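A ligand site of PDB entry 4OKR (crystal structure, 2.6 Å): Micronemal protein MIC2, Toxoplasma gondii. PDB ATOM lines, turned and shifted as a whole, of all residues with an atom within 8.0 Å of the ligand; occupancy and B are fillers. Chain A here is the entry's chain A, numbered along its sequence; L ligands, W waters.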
ATOM      1  N   CYS A 207      24.139 -17.786 -22.865  1.00  0.00           N
ATOM      2  CA  CYS A 207      22.912 -17.015 -22.852  1.00  0.00           C
ATOM      3  C   CYS A 207      23.219 -15.531 -22.977  1.00  0.00           C
ATOM      4  O   CYS A 207      24.308 -15.086 -22.611  1.00  0.00           O
ATOM      5  CB  CYS A 207      22.122 -17.268 -21.563  1.00  0.00           C
ATOM      6  SG  CYS A 207      21.899 -19.014 -21.131  1.00  0.00           S
ATOM      7  N   SER A 208      22.268 -14.770 -23.494  1.00  0.00           N
ATOM      8  CA  SER A 208      22.385 -13.323 -23.503  1.00  0.00           C
ATOM      9  C   SER A 208      22.130 -12.790 -22.101  1.00  0.00           C
ATOM     10  O   SER A 208      21.709 -13.539 -21.214  1.00  0.00           O
ATOM     11  CB  SER A 208      21.408 -12.707 -24.501  1.00  0.00           C
ATOM     12  OG  SER A 208      20.074 -12.872 -24.074  1.00  0.00           O
ATOM     13  N   ASP A 209      22.374 -11.498 -21.902  1.00  0.00           N
ATOM     14  CA  ASP A 209      22.063 -10.886 -20.616  1.00  0.00           C
ATOM     15  C   ASP A 209      20.561 -10.671 -20.493  1.00  0.00           C
ATOM     16  O   ASP A 209      19.860 -10.597 -21.499  1.00  0.00           O
ATOM     17  CB  ASP A 209      22.812  -9.550 -20.454  1.00  0.00           C
ATOM     18  CG  ASP A 209      24.298  -9.747 -20.206  1.00  0.00           C
ATOM     19  OD1 ASP A 209      24.653 -10.494 -19.274  1.00  0.00           O
ATOM     20  OD2 ASP A 209      25.113  -9.139 -20.941  1.00  0.00           O
ATOM     21  N   TRP A 210      20.072 -10.589 -19.260  1.00  0.00           N
ATOM     22  CA  TRP A 210      18.655 -10.402 -19.032  1.00  0.00           C
ATOM     23  C   TRP A 210      18.171  -9.066 -19.577  1.00  0.00           C
ATOM     24  O   TRP A 210      18.879  -8.058 -19.516  1.00  0.00           O
ATOM     25  CB  TRP A 210      18.326 -10.492 -17.547  1.00  0.00           C
ATOM     26  CG  TRP A 210      18.539 -11.849 -16.965  1.00  0.00           C
ATOM     27  CD1 TRP A 210      19.546 -12.239 -16.127  1.00  0.00           C
ATOM     28  CD2 TRP A 210      17.740 -13.020 -17.200  1.00  0.00           C
ATOM     29  NE1 TRP A 210      19.411 -13.565 -15.805  1.00  0.00           N
ATOM     30  CE2 TRP A 210      18.315 -14.068 -16.461  1.00  0.00           C
ATOM     31  CE3 TRP A 210      16.595 -13.269 -17.961  1.00  0.00           C
ATOM     32  CZ2 TRP A 210      17.772 -15.355 -16.457  1.00  0.00           C
ATOM     33  CZ3 TRP A 210      16.069 -14.547 -17.963  1.00  0.00           C
ATOM     34  CH2 TRP A 210      16.659 -15.572 -17.212  1.00  0.00           C
ATOM     35  N   SER A 211      16.953  -9.069 -20.103  1.00  0.00           N
ATOM     36  CA  SER A 211      16.290  -7.840 -20.509  1.00  0.00           C
ATOM     37  C   SER A 211      15.836  -7.078 -19.277  1.00  0.00           C
ATOM     38  O   SER A 211      15.795  -7.636 -18.182  1.00  0.00           O
ATOM     39  CB  SER A 211      15.091  -8.126 -21.419  1.00  0.00           C
ATOM     40  OG  SER A 211      14.009  -8.640 -20.669  1.00  0.00           O
ATOM     41  N   TRP A 213      13.397  -5.375 -16.588  1.00  0.00           N
ATOM     42  CA  TRP A 213      12.133  -5.852 -16.048  1.00  0.00           C
ATOM     43  C   TRP A 213      10.966  -5.173 -16.740  1.00  0.00           C
ATOM     44  O   TRP A 213      10.957  -3.957 -16.926  1.00  0.00           O
ATOM     45  CB  TRP A 213      12.072  -5.605 -14.541  1.00  0.00           C
ATOM     46  CG  TRP A 213      13.046  -6.434 -13.745  1.00  0.00           C
ATOM     47  CD1 TRP A 213      14.199  -6.002 -13.170  1.00  0.00           C
ATOM     48  CD2 TRP A 213      12.940  -7.832 -13.445  1.00  0.00           C
ATOM     49  NE1 TRP A 213      14.823  -7.046 -12.524  1.00  0.00           N
ATOM     50  CE2 TRP A 213      14.076  -8.174 -12.676  1.00  0.00           C
ATOM     51  CE3 TRP A 213      12.000  -8.818 -13.747  1.00  0.00           C
ATOM     52  CZ2 TRP A 213      14.288  -9.468 -12.213  1.00  0.00           C
ATOM     53  CZ3 TRP A 213      12.220 -10.108 -13.287  1.00  0.00           C
ATOM     54  CH2 TRP A 213      13.350 -10.421 -12.527  1.00  0.00           C
ATOM     55  N   ARG A 227      11.249 -10.694 -17.265  1.00  0.00           N
ATOM     56  CA  ARG A 227      12.369 -10.383 -18.142  1.00  0.00           C
ATOM     57  C   ARG A 227      12.806 -11.631 -18.908  1.00  0.00           C
ATOM     58  O   ARG A 227      12.566 -12.757 -18.449  1.00  0.00           O
ATOM     59  CB  ARG A 227      13.550  -9.814 -17.341  1.00  0.00           C
ATOM     60  CG  ARG A 227      14.119 -10.751 -16.307  1.00  0.00           C
ATOM     61  CD  ARG A 227      15.269 -10.098 -15.574  1.00  0.00           C
ATOM     62  NE  ARG A 227      15.925 -11.026 -14.653  1.00  0.00           N
ATOM     63  CZ  ARG A 227      17.022 -10.727 -13.957  1.00  0.00           C
ATOM     64  NH1 ARG A 227      17.584  -9.536 -14.090  1.00  0.00           N
ATOM     65  NH2 ARG A 227      17.558 -11.623 -13.138  1.00  0.00           N
ATOM     66  N   THR A 228      13.443 -11.444 -20.055  1.00  0.00           N
ATOM     67  CA  THR A 228      13.812 -12.557 -20.924  1.00  0.00           C
ATOM     68  C   THR A 228      15.265 -12.507 -21.381  1.00  0.00           C
ATOM     69  O   THR A 228      15.966 -11.520 -21.162  1.00  0.00           O
ATOM     70  CB  THR A 228      12.918 -12.598 -22.193  1.00  0.00           C
ATOM     71  OG1 THR A 228      13.156 -11.432 -22.987  1.00  0.00           O
ATOM     72  CG2 THR A 228      11.444 -12.657 -21.814  1.00  0.00           C
ATOM     73  N   ARG A 229      15.712 -13.591 -22.004  1.00  0.00           N
ATOM     74  CA  ARG A 229      17.054 -13.676 -22.579  1.00  0.00           C
ATOM     75  C   ARG A 229      17.104 -14.734 -23.688  1.00  0.00           C
ATOM     76  O   ARG A 229      16.186 -15.541 -23.822  1.00  0.00           O
ATOM     77  CB  ARG A 229      18.085 -13.996 -21.492  1.00  0.00           C
ATOM     78  CG  ARG A 229      18.000 -15.414 -20.951  1.00  0.00           C
ATOM     79  CD  ARG A 229      18.998 -15.622 -19.823  1.00  0.00           C
ATOM     80  NE  ARG A 229      18.860 -16.951 -19.232  1.00  0.00           N
ATOM     81  CZ  ARG A 229      19.645 -17.415 -18.260  1.00  0.00           C
ATOM     82  NH1 ARG A 229      20.608 -16.662 -17.760  1.00  0.00           N
ATOM     83  NH2 ARG A 229      19.450 -18.640 -17.783  1.00  0.00           N
ATOM     84  N   GLU A 261      12.404 -14.949 -16.195  1.00  0.00           N
ATOM     85  CA  GLU A 261      12.304 -14.803 -14.753  1.00  0.00           C
ATOM     86  C   GLU A 261      11.131 -13.896 -14.400  1.00  0.00           C
ATOM     87  O   GLU A 261      10.913 -12.872 -15.055  1.00  0.00           O
ATOM     88  CB  GLU A 261      13.593 -14.236 -14.160  1.00  0.00           C
ATOM     89  CG  GLU A 261      14.711 -15.256 -14.003  1.00  0.00           C
ATOM     90  CD  GLU A 261      15.952 -14.657 -13.361  1.00  0.00           C
ATOM     91  OE1 GLU A 261      16.993 -15.345 -13.312  1.00  0.00           O
ATOM     92  OE2 GLU A 261      15.874 -13.500 -12.894  1.00  0.00           O
HETATM   93  C1  LIG L   1      20.520 -11.502 -15.441  1.00  0.00           C
HETATM   94  C2  LIG L   1      21.938 -11.909 -15.869  1.00  0.00           C
HETATM   95  C3  LIG L   1      22.990 -11.150 -15.052  1.00  0.00           C
HETATM   96  C4  LIG L   1      22.680 -11.108 -13.521  1.00  0.00           C
HETATM   97  C5  LIG L   1      21.184 -10.796 -13.229  1.00  0.00           C
HETATM   98  C6  LIG L   1      20.814  -9.326 -13.399  1.00  0.00           C
HETATM   99  O1  LIG L   1      22.194 -11.580 -17.236  1.00  0.00           O
HETATM  100  O2  LIG L   1      23.211  -9.832 -15.556  1.00  0.00           O
HETATM  101  O3  LIG L   1      23.048 -12.343 -12.920  1.00  0.00           O
HETATM  102  O4  LIG L   1      20.310 -11.597 -14.068  1.00  0.00           O
HETATM  103  O5  LIG L   1      21.520  -8.566 -12.424  1.00  0.00           O
HETATM  104  O   HOH W   1      22.324 -13.927 -18.411  1.00  0.00           O
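The aromatic ring (CD1) of Trp 210 is bonded to a carbon (C1) of the ligand (1.4 Å).
The guanidinium group (NH2) of Arg 227 lies within hydrogen-bond range of an oxygen (O4) of the ligand.
N of Trp 210 sits close to O1 of the ligand (3.1 Å).
The side-chain carboxylate (OD1) of Asp 209 sits at hydrogen-bond distance from an oxygen (O1) of the ligand (3.4 Å).
The guanidinium group of Arg 227 is in salt-bridge range of the side-chain carboxylate of Glu 261, at 2.5 Å.
Hydrophobic or aromatic side chains that line the ligand: Trp 210.
Of the 10 residues printed, 3 come within 4 Å of the ligand.
The nearest printed residue that does not touch the ligand is Ser 208 (4.5 Å).
Water W1 lies within hydrogen-bond range of an oxygen (O1) of the ligand (2.6 Å), the backbone carbonyl oxygen (O) of Ser 208 (2.9 Å) and the guanidinium group (NH1) of Arg 229 (3.3 Å).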
